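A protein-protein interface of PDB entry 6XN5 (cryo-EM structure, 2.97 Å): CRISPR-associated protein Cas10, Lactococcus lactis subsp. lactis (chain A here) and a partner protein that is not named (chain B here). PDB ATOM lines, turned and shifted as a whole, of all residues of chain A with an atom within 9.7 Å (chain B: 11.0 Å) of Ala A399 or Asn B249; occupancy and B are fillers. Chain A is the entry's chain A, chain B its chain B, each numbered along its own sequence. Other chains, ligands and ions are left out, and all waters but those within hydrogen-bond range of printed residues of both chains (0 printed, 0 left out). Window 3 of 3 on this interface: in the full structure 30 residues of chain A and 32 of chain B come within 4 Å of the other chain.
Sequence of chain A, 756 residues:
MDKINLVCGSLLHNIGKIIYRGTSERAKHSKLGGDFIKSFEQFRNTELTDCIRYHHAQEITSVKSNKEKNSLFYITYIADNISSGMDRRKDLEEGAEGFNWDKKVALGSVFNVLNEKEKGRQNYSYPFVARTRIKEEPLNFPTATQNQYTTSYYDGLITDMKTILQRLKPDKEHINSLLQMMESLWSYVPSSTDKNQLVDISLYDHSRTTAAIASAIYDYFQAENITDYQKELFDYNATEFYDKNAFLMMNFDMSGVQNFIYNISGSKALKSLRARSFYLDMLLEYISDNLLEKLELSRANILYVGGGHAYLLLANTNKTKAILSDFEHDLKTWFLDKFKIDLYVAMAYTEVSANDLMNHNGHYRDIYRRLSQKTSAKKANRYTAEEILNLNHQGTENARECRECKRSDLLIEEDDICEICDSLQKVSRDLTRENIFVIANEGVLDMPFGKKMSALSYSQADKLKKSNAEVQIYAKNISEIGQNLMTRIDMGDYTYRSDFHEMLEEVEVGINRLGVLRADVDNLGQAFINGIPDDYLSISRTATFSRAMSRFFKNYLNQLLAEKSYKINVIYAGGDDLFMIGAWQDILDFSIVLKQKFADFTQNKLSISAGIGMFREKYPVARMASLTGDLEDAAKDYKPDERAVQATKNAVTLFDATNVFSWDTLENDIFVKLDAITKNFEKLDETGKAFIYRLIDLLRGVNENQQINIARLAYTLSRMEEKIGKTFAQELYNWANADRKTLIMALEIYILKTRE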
ATOM      1  N   THR A 396       6.171   4.865 -23.258  1.00  0.00           N
ATOM      2  CA  THR A 396       6.665   5.762 -24.287  1.00  0.00           C
ATOM      3  C   THR A 396       5.811   7.019 -24.276  1.00  0.00           C
ATOM      4  O   THR A 396       4.836   7.121 -23.528  1.00  0.00           O
ATOM      5  CB  THR A 396       6.629   5.105 -25.672  1.00  0.00           C
ATOM      6  OG1 THR A 396       5.273   4.815 -26.028  1.00  0.00           O
ATOM      7  CG2 THR A 396       7.433   3.818 -25.684  1.00  0.00           C
ATOM      8  N   GLU A 397       6.179   7.980 -25.114  1.00  0.00           N
ATOM      9  CA  GLU A 397       5.368   9.161 -25.370  1.00  0.00           C
ATOM     10  C   GLU A 397       4.820   9.063 -26.782  1.00  0.00           C
ATOM     11  O   GLU A 397       5.587   8.869 -27.730  1.00  0.00           O
ATOM     12  CB  GLU A 397       6.180  10.446 -25.242  1.00  0.00           C
ATOM     13  CG  GLU A 397       7.163  10.490 -24.109  1.00  0.00           C
ATOM     14  CD  GLU A 397       7.871  11.824 -24.044  1.00  0.00           C
ATOM     15  OE1 GLU A 397       7.456  12.752 -24.768  1.00  0.00           O
ATOM     16  OE2 GLU A 397       8.855  11.940 -23.287  1.00  0.00           O
ATOM     17  N   ASN A 398       3.506   9.211 -26.925  1.00  0.00           N
ATOM     18  CA  ASN A 398       2.890   9.143 -28.242  1.00  0.00           C
ATOM     19  C   ASN A 398       1.593   9.942 -28.291  1.00  0.00           C
ATOM     20  O   ASN A 398       0.887  10.064 -27.291  1.00  0.00           O
ATOM     21  CB  ASN A 398       2.719   7.679 -28.696  1.00  0.00           C
ATOM     22  CG  ASN A 398       1.808   6.848 -27.802  1.00  0.00           C
ATOM     23  OD1 ASN A 398       1.173   7.329 -26.874  1.00  0.00           O
ATOM     24  ND2 ASN A 398       1.758   5.557 -28.095  1.00  0.00           N
ATOM     25  N   ALA A 399       1.334  10.547 -29.446  1.00  0.00           N
ATOM     26  CA  ALA A 399       0.169  11.410 -29.620  1.00  0.00           C
ATOM     27  C   ALA A 399      -0.983  10.644 -30.264  1.00  0.00           C
ATOM     28  O   ALA A 399      -1.642  11.122 -31.182  1.00  0.00           O
ATOM     29  CB  ALA A 399       0.546  12.630 -30.449  1.00  0.00           C
ATOM     30  N   ARG A 400      -1.245   9.454 -29.737  1.00  0.00           N
ATOM     31  CA  ARG A 400      -2.302   8.605 -30.266  1.00  0.00           C
ATOM     32  C   ARG A 400      -2.867   7.762 -29.138  1.00  0.00           C
ATOM     33  O   ARG A 400      -2.181   7.451 -28.164  1.00  0.00           O
ATOM     34  CB  ARG A 400      -1.802   7.707 -31.400  1.00  0.00           C
ATOM     35  CG  ARG A 400      -1.881   8.319 -32.783  1.00  0.00           C
ATOM     36  CD  ARG A 400      -1.426   7.342 -33.843  1.00  0.00           C
ATOM     37  NE  ARG A 400      -2.463   6.375 -34.166  1.00  0.00           N
ATOM     38  CZ  ARG A 400      -2.226   5.196 -34.723  1.00  0.00           C
ATOM     39  NH1 ARG A 400      -0.985   4.838 -35.011  1.00  0.00           N
ATOM     40  NH2 ARG A 400      -3.228   4.375 -34.990  1.00  0.00           N
ATOM     41  N   GLU A 401      -4.124   7.375 -29.304  1.00  0.00           N
ATOM     42  CA  GLU A 401      -4.846   6.645 -28.275  1.00  0.00           C
ATOM     43  C   GLU A 401      -6.055   6.004 -28.930  1.00  0.00           C
ATOM     44  O   GLU A 401      -6.593   6.520 -29.910  1.00  0.00           O
ATOM     45  CB  GLU A 401      -5.273   7.582 -27.149  1.00  0.00           C
ATOM     46  CG  GLU A 401      -5.697   6.904 -25.892  1.00  0.00           C
ATOM     47  CD  GLU A 401      -6.335   7.864 -24.938  1.00  0.00           C
ATOM     48  OE1 GLU A 401      -6.545   9.032 -25.319  1.00  0.00           O
ATOM     49  OE2 GLU A 401      -6.627   7.446 -23.806  1.00  0.00           O
ATOM     50  N   CYS A 402      -6.484   4.874 -28.379  1.00  0.00           N
ATOM     51  CA  CYS A 402      -7.685   4.227 -28.874  1.00  0.00           C
ATOM     52  C   CYS A 402      -8.931   5.042 -28.547  1.00  0.00           C
ATOM     53  O   CYS A 402      -8.977   5.799 -27.577  1.00  0.00           O
ATOM     54  CB  CYS A 402      -7.849   2.838 -28.279  1.00  0.00           C
ATOM     55  SG  CYS A 402      -9.515   2.257 -28.553  1.00  0.00           S
ATOM     56  N   ARG A 407      -5.966   2.823 -24.594  1.00  0.00           N
ATOM     57  CA  ARG A 407      -4.555   2.555 -24.387  1.00  0.00           C
ATOM     58  C   ARG A 407      -3.784   3.001 -25.615  1.00  0.00           C
ATOM     59  O   ARG A 407      -4.343   3.131 -26.706  1.00  0.00           O
ATOM     60  CB  ARG A 407      -4.309   1.073 -24.122  1.00  0.00           C
ATOM     61  CG  ARG A 407      -4.664   0.200 -25.292  1.00  0.00           C
ATOM     62  CD  ARG A 407      -4.644  -1.260 -24.946  1.00  0.00           C
ATOM     63  NE  ARG A 407      -3.292  -1.758 -24.759  1.00  0.00           N
ATOM     64  CZ  ARG A 407      -3.013  -2.892 -24.135  1.00  0.00           C
ATOM     65  NH1 ARG A 407      -3.999  -3.630 -23.649  1.00  0.00           N
ATOM     66  NH2 ARG A 407      -1.760  -3.295 -24.002  1.00  0.00           N
ATOM     67  N   SER A 408      -2.493   3.251 -25.433  1.00  0.00           N
ATOM     68  CA  SER A 408      -1.658   3.751 -26.511  1.00  0.00           C
ATOM     69  C   SER A 408      -0.666   2.726 -27.031  1.00  0.00           C
ATOM     70  O   SER A 408       0.212   3.075 -27.822  1.00  0.00           O
ATOM     71  CB  SER A 408      -0.925   5.002 -26.058  1.00  0.00           C
ATOM     72  OG  SER A 408      -1.768   6.125 -26.189  1.00  0.00           O
ATOM     73  N   LEU A 411      -1.631  -0.272 -31.066  1.00  0.00           N
ATOM     74  CA  LEU A 411      -2.514   0.471 -31.945  1.00  0.00           C
ATOM     75  C   LEU A 411      -2.319  -0.006 -33.374  1.00  0.00           C
ATOM     76  O   LEU A 411      -1.224  -0.423 -33.756  1.00  0.00           O
ATOM     77  CB  LEU A 411      -2.234   1.968 -31.855  1.00  0.00           C
ATOM     78  CG  LEU A 411      -2.621   2.665 -30.556  1.00  0.00           C
ATOM     79  CD1 LEU A 411      -2.249   4.115 -30.640  1.00  0.00           C
ATOM     80  CD2 LEU A 411      -4.094   2.520 -30.283  1.00  0.00           C
ATOM     81  N   ASP A 416      -6.897   4.743 -35.106  1.00  0.00           N
ATOM     82  CA  ASP A 416      -6.509   4.891 -33.704  1.00  0.00           C
ATOM     83  C   ASP A 416      -7.356   3.962 -32.836  1.00  0.00           C
ATOM     84  O   ASP A 416      -8.347   4.348 -32.217  1.00  0.00           O
ATOM     85  CB  ASP A 416      -6.632   6.346 -33.273  1.00  0.00           C
ATOM     86  CG  ASP A 416      -7.935   6.982 -33.714  1.00  0.00           C
ATOM     87  OD1 ASP A 416      -8.723   6.311 -34.411  1.00  0.00           O
ATOM     88  OD2 ASP A 416      -8.174   8.151 -33.357  1.00  0.00           O
ATOM     89  N   GLY B 239      -1.550   9.945 -18.658  1.00  0.00           N
ATOM     90  CA  GLY B 239      -2.427  10.940 -19.235  1.00  0.00           C
ATOM     91  C   GLY B 239      -1.747  11.823 -20.259  1.00  0.00           C
ATOM     92  O   GLY B 239      -0.654  11.509 -20.727  1.00  0.00           O
ATOM     93  N   PHE B 240      -2.379  12.937 -20.608  1.00  0.00           N
ATOM     94  CA  PHE B 240      -1.825  13.878 -21.568  1.00  0.00           C
ATOM     95  C   PHE B 240      -1.092  14.993 -20.843  1.00  0.00           C
ATOM     96  O   PHE B 240      -1.433  15.358 -19.718  1.00  0.00           O
ATOM     97  CB  PHE B 240      -2.917  14.491 -22.431  1.00  0.00           C
ATOM     98  CG  PHE B 240      -3.421  13.599 -23.518  1.00  0.00           C
ATOM     99  CD1 PHE B 240      -4.355  12.619 -23.247  1.00  0.00           C
ATOM    100  CD2 PHE B 240      -2.993  13.767 -24.818  1.00  0.00           C
ATOM    101  CE1 PHE B 240      -4.834  11.814 -24.250  1.00  0.00           C
ATOM    102  CE2 PHE B 240      -3.471  12.970 -25.827  1.00  0.00           C
ATOM    103  CZ  PHE B 240      -4.395  11.994 -25.546  1.00  0.00           C
ATOM    104  N   VAL B 241      -0.088  15.540 -21.505  1.00  0.00           N
ATOM    105  CA  VAL B 241       0.681  16.643 -20.948  1.00  0.00           C
ATOM    106  C   VAL B 241      -0.134  17.922 -21.064  1.00  0.00           C
ATOM    107  O   VAL B 241      -0.660  18.242 -22.134  1.00  0.00           O
ATOM    108  CB  VAL B 241       2.029  16.773 -21.665  1.00  0.00           C
ATOM    109  CG1 VAL B 241       2.861  17.841 -21.028  1.00  0.00           C
ATOM    110  CG2 VAL B 241       2.752  15.457 -21.633  1.00  0.00           C
ATOM    111  N   GLN B 242      -0.238  18.656 -19.964  1.00  0.00           N
ATOM    112  CA  GLN B 242      -0.983  19.908 -19.900  1.00  0.00           C
ATOM    113  C   GLN B 242       0.028  21.043 -19.787  1.00  0.00           C
ATOM    114  O   GLN B 242       0.574  21.294 -18.709  1.00  0.00           O
ATOM    115  CB  GLN B 242      -1.953  19.888 -18.723  1.00  0.00           C
ATOM    116  CG  GLN B 242      -2.608  21.214 -18.401  1.00  0.00           C
ATOM    117  CD  GLN B 242      -3.765  21.062 -17.464  1.00  0.00           C
ATOM    118  OE1 GLN B 242      -4.344  19.992 -17.351  1.00  0.00           O
ATOM    119  NE2 GLN B 242      -4.104  22.132 -16.767  1.00  0.00           N
ATOM    120  N   SER B 243       0.298  21.697 -20.911  1.00  0.00           N
ATOM    121  CA  SER B 243       1.142  22.885 -20.975  1.00  0.00           C
ATOM    122  C   SER B 243       0.886  23.568 -22.310  1.00  0.00           C
ATOM    123  O   SER B 243      -0.054  23.226 -23.032  1.00  0.00           O
ATOM    124  CB  SER B 243       2.624  22.541 -20.823  1.00  0.00           C
ATOM    125  OG  SER B 243       3.120  22.005 -22.027  1.00  0.00           O
ATOM    126  N   ASP B 244       1.731  24.540 -22.642  1.00  0.00           N
ATOM    127  CA  ASP B 244       1.720  25.134 -23.964  1.00  0.00           C
ATOM    128  C   ASP B 244       3.040  24.993 -24.693  1.00  0.00           C
ATOM    129  O   ASP B 244       3.057  25.083 -25.924  1.00  0.00           O
ATOM    130  CB  ASP B 244       1.382  26.624 -23.903  1.00  0.00           C
ATOM    131  CG  ASP B 244      -0.034  26.882 -23.497  1.00  0.00           C
ATOM    132  OD1 ASP B 244      -0.898  26.028 -23.779  1.00  0.00           O
ATOM    133  OD2 ASP B 244      -0.287  27.974 -22.949  1.00  0.00           O
ATOM    134  N   THR B 245       4.141  24.785 -23.984  1.00  0.00           N
ATOM    135  CA  THR B 245       5.454  24.840 -24.602  1.00  0.00           C
ATOM    136  C   THR B 245       5.993  23.449 -24.900  1.00  0.00           C
ATOM    137  O   THR B 245       7.133  23.305 -25.331  1.00  0.00           O
ATOM    138  CB  THR B 245       6.432  25.613 -23.723  1.00  0.00           C
ATOM    139  OG1 THR B 245       6.477  25.020 -22.422  1.00  0.00           O
ATOM    140  CG2 THR B 245       5.990  27.057 -23.597  1.00  0.00           C
ATOM    141  N   TYR B 246       5.187  22.417 -24.701  1.00  0.00           N
ATOM    142  CA  TYR B 246       5.617  21.043 -24.922  1.00  0.00           C
ATOM    143  C   TYR B 246       5.110  20.595 -26.285  1.00  0.00           C
ATOM    144  O   TYR B 246       3.903  20.424 -26.479  1.00  0.00           O
ATOM    145  CB  TYR B 246       5.105  20.132 -23.809  1.00  0.00           C
ATOM    146  CG  TYR B 246       5.790  18.791 -23.706  1.00  0.00           C
ATOM    147  CD1 TYR B 246       5.436  17.740 -24.530  1.00  0.00           C
ATOM    148  CD2 TYR B 246       6.771  18.569 -22.758  1.00  0.00           C
ATOM    149  CE1 TYR B 246       6.054  16.524 -24.434  1.00  0.00           C
ATOM    150  CE2 TYR B 246       7.395  17.350 -22.655  1.00  0.00           C
ATOM    151  CZ  TYR B 246       7.029  16.336 -23.500  1.00  0.00           C
ATOM    152  OH  TYR B 246       7.638  15.112 -23.412  1.00  0.00           O
ATOM    153  N   ALA B 247       6.031  20.453 -27.236  1.00  0.00           N
ATOM    154  CA  ALA B 247       5.907  19.651 -28.451  1.00  0.00           C
ATOM    155  C   ALA B 247       4.814  20.085 -29.422  1.00  0.00           C
ATOM    156  O   ALA B 247       4.446  19.283 -30.282  1.00  0.00           O
ATOM    157  CB  ALA B 247       5.690  18.171 -28.120  1.00  0.00           C
ATOM    158  N   THR B 248       4.256  21.297 -29.282  1.00  0.00           N
ATOM    159  CA  THR B 248       3.346  22.005 -30.221  1.00  0.00           C
ATOM    160  C   THR B 248       2.133  21.179 -30.701  1.00  0.00           C
ATOM    161  O   THR B 248       1.445  21.578 -31.645  1.00  0.00           O
ATOM    162  CB  THR B 248       4.100  22.616 -31.428  1.00  0.00           C
ATOM    163  OG1 THR B 248       3.246  23.558 -32.085  1.00  0.00           O
ATOM    164  CG2 THR B 248       4.553  21.602 -32.489  1.00  0.00           C
ATOM    165  N   ASN B 249       1.811  20.077 -30.030  1.00  0.00           N
ATOM    166  CA  ASN B 249       0.563  19.344 -30.198  1.00  0.00           C
ATOM    167  C   ASN B 249       0.359  18.505 -28.947  1.00  0.00           C
ATOM    168  O   ASN B 249       1.291  18.296 -28.168  1.00  0.00           O
ATOM    169  CB  ASN B 249       0.552  18.477 -31.467  1.00  0.00           C
ATOM    170  CG  ASN B 249       1.429  17.239 -31.362  1.00  0.00           C
ATOM    171  OD1 ASN B 249       2.497  17.256 -30.756  1.00  0.00           O
ATOM    172  ND2 ASN B 249       0.980  16.154 -31.982  1.00  0.00           N
ATOM    173  N   LEU B 250      -0.873  18.050 -28.752  1.00  0.00           N
ATOM    174  CA  LEU B 250      -1.219  17.227 -27.601  1.00  0.00           C
ATOM    175  C   LEU B 250      -0.501  15.886 -27.664  1.00  0.00           C
ATOM    176  O   LEU B 250      -0.414  15.259 -28.719  1.00  0.00           O
ATOM    177  CB  LEU B 250      -2.723  17.001 -27.563  1.00  0.00           C
ATOM    178  CG  LEU B 250      -3.654  17.897 -26.758  1.00  0.00           C
ATOM    179  CD1 LEU B 250      -3.582  19.328 -27.185  1.00  0.00           C
ATOM    180  CD2 LEU B 250      -5.034  17.394 -27.031  1.00  0.00           C
ATOM    181  N   VAL B 251       0.015  15.443 -26.521  1.00  0.00           N
ATOM    182  CA  VAL B 251       0.854  14.250 -26.480  1.00  0.00           C
ATOM    183  C   VAL B 251       0.706  13.599 -25.109  1.00  0.00           C
ATOM    184  O   VAL B 251       0.536  14.281 -24.096  1.00  0.00           O
ATOM    185  CB  VAL B 251       2.319  14.609 -26.837  1.00  0.00           C
ATOM    186  CG1 VAL B 251       2.900  15.565 -25.845  1.00  0.00           C
ATOM    187  CG2 VAL B 251       3.194  13.376 -26.979  1.00  0.00           C
ATOM    188  N   LYS B 252       0.714  12.267 -25.092  1.00  0.00           N
ATOM    189  CA  LYS B 252       0.556  11.501 -23.866  1.00  0.00           C
ATOM    190  C   LYS B 252       1.902  11.260 -23.209  1.00  0.00           C
ATOM    191  O   LYS B 252       2.862  10.863 -23.874  1.00  0.00           O
ATOM    192  CB  LYS B 252      -0.115  10.163 -24.149  1.00  0.00           C
ATOM    193  CG  LYS B 252      -1.564  10.286 -24.391  1.00  0.00           C
ATOM    194  CD  LYS B 252      -2.223   8.974 -24.676  1.00  0.00           C
ATOM    195  CE  LYS B 252      -2.181   8.096 -23.466  1.00  0.00           C
ATOM    196  NZ  LYS B 252      -2.866   8.762 -22.349  1.00  0.00           N
ATOM    197  N   LYS B 253       1.961  11.471 -21.901  1.00  0.00           N
ATOM    198  CA  LYS B 253       3.187  11.245 -21.165  1.00  0.00           C
ATOM    199  C   LYS B 253       3.418   9.750 -20.977  1.00  0.00           C
ATOM    200  O   LYS B 253       2.579   8.916 -21.316  1.00  0.00           O
ATOM    201  CB  LYS B 253       3.133  11.965 -19.822  1.00  0.00           C
ATOM    202  CG  LYS B 253       2.085  11.441 -18.877  1.00  0.00           C
ATOM    203  CD  LYS B 253       2.121  12.176 -17.555  1.00  0.00           C
ATOM    204  CE  LYS B 253       1.597  13.586 -17.641  1.00  0.00           C
ATOM    205  NZ  LYS B 253       0.157  13.612 -17.953  1.00  0.00           N
ATOM    206  N   GLN B 254       4.589   9.418 -20.444  1.00  0.00           N
ATOM    207  CA  GLN B 254       4.933   8.027 -20.200  1.00  0.00           C
ATOM    208  C   GLN B 254       4.075   7.449 -19.084  1.00  0.00           C
ATOM    209  O   GLN B 254       3.867   8.081 -18.048  1.00  0.00           O
ATOM    210  CB  GLN B 254       6.406   7.908 -19.831  1.00  0.00           C
ATOM    211  CG  GLN B 254       7.325   7.734 -21.011  1.00  0.00           C
ATOM    212  CD  GLN B 254       8.775   7.704 -20.603  1.00  0.00           C
ATOM    213  OE1 GLN B 254       9.164   6.955 -19.710  1.00  0.00           O
ATOM    214  NE2 GLN B 254       9.589   8.521 -21.255  1.00  0.00           N
ATOM    215  N   VAL B 276       8.409  11.766 -16.805  1.00  0.00           N
ATOM    216  CA  VAL B 276       7.567  11.056 -17.755  1.00  0.00           C
ATOM    217  C   VAL B 276       7.503  11.778 -19.096  1.00  0.00           C
ATOM    218  O   VAL B 276       6.909  11.276 -20.039  1.00  0.00           O
ATOM    219  CB  VAL B 276       6.160  10.832 -17.178  1.00  0.00           C
ATOM    220  CG1 VAL B 276       6.192   9.749 -16.132  1.00  0.00           C
ATOM    221  CG2 VAL B 276       5.683  12.100 -16.567  1.00  0.00           C
ATOM    222  N   LYS B 279      10.765  14.110 -24.516  1.00  0.00           N
ATOM    223  CA  LYS B 279      10.855  14.612 -25.887  1.00  0.00           C
ATOM    224  C   LYS B 279      10.060  15.907 -26.044  1.00  0.00           C
ATOM    225  O   LYS B 279       9.146  16.016 -26.856  1.00  0.00           O
ATOM    226  CB  LYS B 279      10.379  13.545 -26.866  1.00  0.00           C
ATOM    227  CG  LYS B 279      11.214  12.282 -26.849  1.00  0.00           C
ATOM    228  CD  LYS B 279      10.796  11.325 -27.944  1.00  0.00           C
ATOM    229  CE  LYS B 279       9.484  10.647 -27.618  1.00  0.00           C
ATOM    230  NZ  LYS B 279       9.619   9.732 -26.457  1.00  0.00           N
ATOM    231  N   GLY B 280      10.432  16.906 -25.256  1.00  0.00           N
ATOM    232  CA  GLY B 280       9.740  18.181 -25.285  1.00  0.00           C
ATOM    233  C   GLY B 280      10.667  19.279 -24.822  1.00  0.00           C
ATOM    234  O   GLY B 280      11.827  19.037 -24.482  1.00  0.00           O
ATOM    235  N   ASN B 281      10.139  20.503 -24.819  1.00  0.00           N
ATOM    236  CA  ASN B 281      10.978  21.652 -24.491  1.00  0.00           C
ATOM    237  C   ASN B 281      11.225  21.760 -22.992  1.00  0.00           C
ATOM    238  O   ASN B 281      12.215  22.362 -22.564  1.00  0.00           O
ATOM    239  CB  ASN B 281      10.351  22.932 -25.030  1.00  0.00           C
ATOM    240  CG  ASN B 281      10.120  22.877 -26.521  1.00  0.00           C
ATOM    241  OD1 ASN B 281      11.055  22.677 -27.292  1.00  0.00           O
ATOM    242  ND2 ASN B 281       8.875  23.052 -26.937  1.00  0.00           N
ATOM    243  N   HIS B 282      10.340  21.199 -22.185  1.00  0.00           N
ATOM    244  CA  HIS B 282      10.464  21.201 -20.739  1.00  0.00           C
ATOM    245  C   HIS B 282      10.176  19.807 -20.204  1.00  0.00           C
ATOM    246  O   HIS B 282       9.440  19.039 -20.830  1.00  0.00           O
ATOM    247  CB  HIS B 282       9.496  22.223 -20.130  1.00  0.00           C
ATOM    248  CG  HIS B 282       8.061  21.827 -20.223  1.00  0.00           C
ATOM    249  ND1 HIS B 282       7.437  21.060 -19.266  1.00  0.00           N
ATOM    250  CD2 HIS B 282       7.125  22.097 -21.158  1.00  0.00           C
ATOM    251  CE1 HIS B 282       6.178  20.870 -19.611  1.00  0.00           C
ATOM    252  NE2 HIS B 282       5.962  21.491 -20.754  1.00  0.00           N
ATOM    253  N   VAL B 284       8.559  16.827 -17.767  1.00  0.00           N
ATOM    254  CA  VAL B 284       7.275  16.545 -17.136  1.00  0.00           C
ATOM    255  C   VAL B 284       7.542  15.586 -15.990  1.00  0.00           C
ATOM    256  O   VAL B 284       8.160  14.536 -16.192  1.00  0.00           O
ATOM    257  CB  VAL B 284       6.262  15.939 -18.121  1.00  0.00           C
ATOM    258  CG1 VAL B 284       4.946  15.688 -17.436  1.00  0.00           C
ATOM    259  CG2 VAL B 284       6.057  16.857 -19.293  1.00  0.00           C
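Ala A399 touches two residues of chain B. Of chain A, only Ala A399 (3.9 Å) comes within 4 Å of Asn B249. Ala B247 touches none of the printed residues of chain A. No residue of chain A comes within 4 Å of Thr B248. Of the printed residues of chain A, Val B276 touches Glu A397. Of the printed residues of chain B, Thr A396 touches Lys B253 and Gln B254. Of the printed residues of chain B, Glu A397 touches Tyr B246 (2.7 Å), Lys B252 (3.4 Å), Val B276 (3.8 Å) and Lys B279 (3.1 Å). The nearest residue of chain B that does not touch Ala A399 is Val B251 (4.2 Å). The nearest residue of chain A that does not touch Asn B249 is Asn A398 (7.3 Å). The nearest printed residue of chain A that does not touch Leu B250 is Asn A398 (5.5 Å).
OH of Tyr B246 sits at hydrogen-bond distance from OE1 of Glu A397, at 2.7 Å. The side-chain carboxylate (OE2) of Glu A397 is in salt-bridge range of the side-chain amino group (NZ) of Lys B279 (3.9 Å). N of Lys B252 is in hydrogen-bond range of O of Asn A398, at 3.1 Å.
Of the 22 printed residues of chain B, 9 touch a printed residue of chain A. Hydrophobic or aromatic side chains of chain A that line the printed part of chain B: Ala A399. Among the printed residues, Asp or Glu carboxylates within 4 Å of a Lys or Arg side-chain nitrogen of the other chain: Glu A397 with Lys B279.
The backbone carbonyl oxygen of Val B276 sits at hydrogen-bond distance from the backbone NH of Gln B254 (3.0 Å). The backbone carbonyl oxygen (O) of Ala B247 sits close to the side-chain amide oxygen (OD1) of Asn B249 (2.9 Å). The side-chain hydroxyl of Ser A408 is in hydrogen-bond range of the backbone carbonyl oxygen of Arg A400 (2.4 Å). OH of Tyr B246 lies within hydrogen-bond range of N of Lys B279, at 3.5 Å. OG of Ser B243 sits close to N of Tyr B246 (3.4 Å). The side-chain amide nitrogen (ND2) of Asn A398 lies within hydrogen-bond range of the backbone carbonyl oxygen (O) of Ser A408, at 2.9 Å.
Among the printed residues, merely in contact across the chains: Thr A396 with Lys B253, Thr A396 with Gln B254, Glu A397 with Lys B252, Glu A397 with Val B276, Ala A399 with Asn B249, Ala A399 with Leu B250, Arg A400 with Lys B252, Glu A401 with Phe B240 and Ser A408 with Lys B252.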
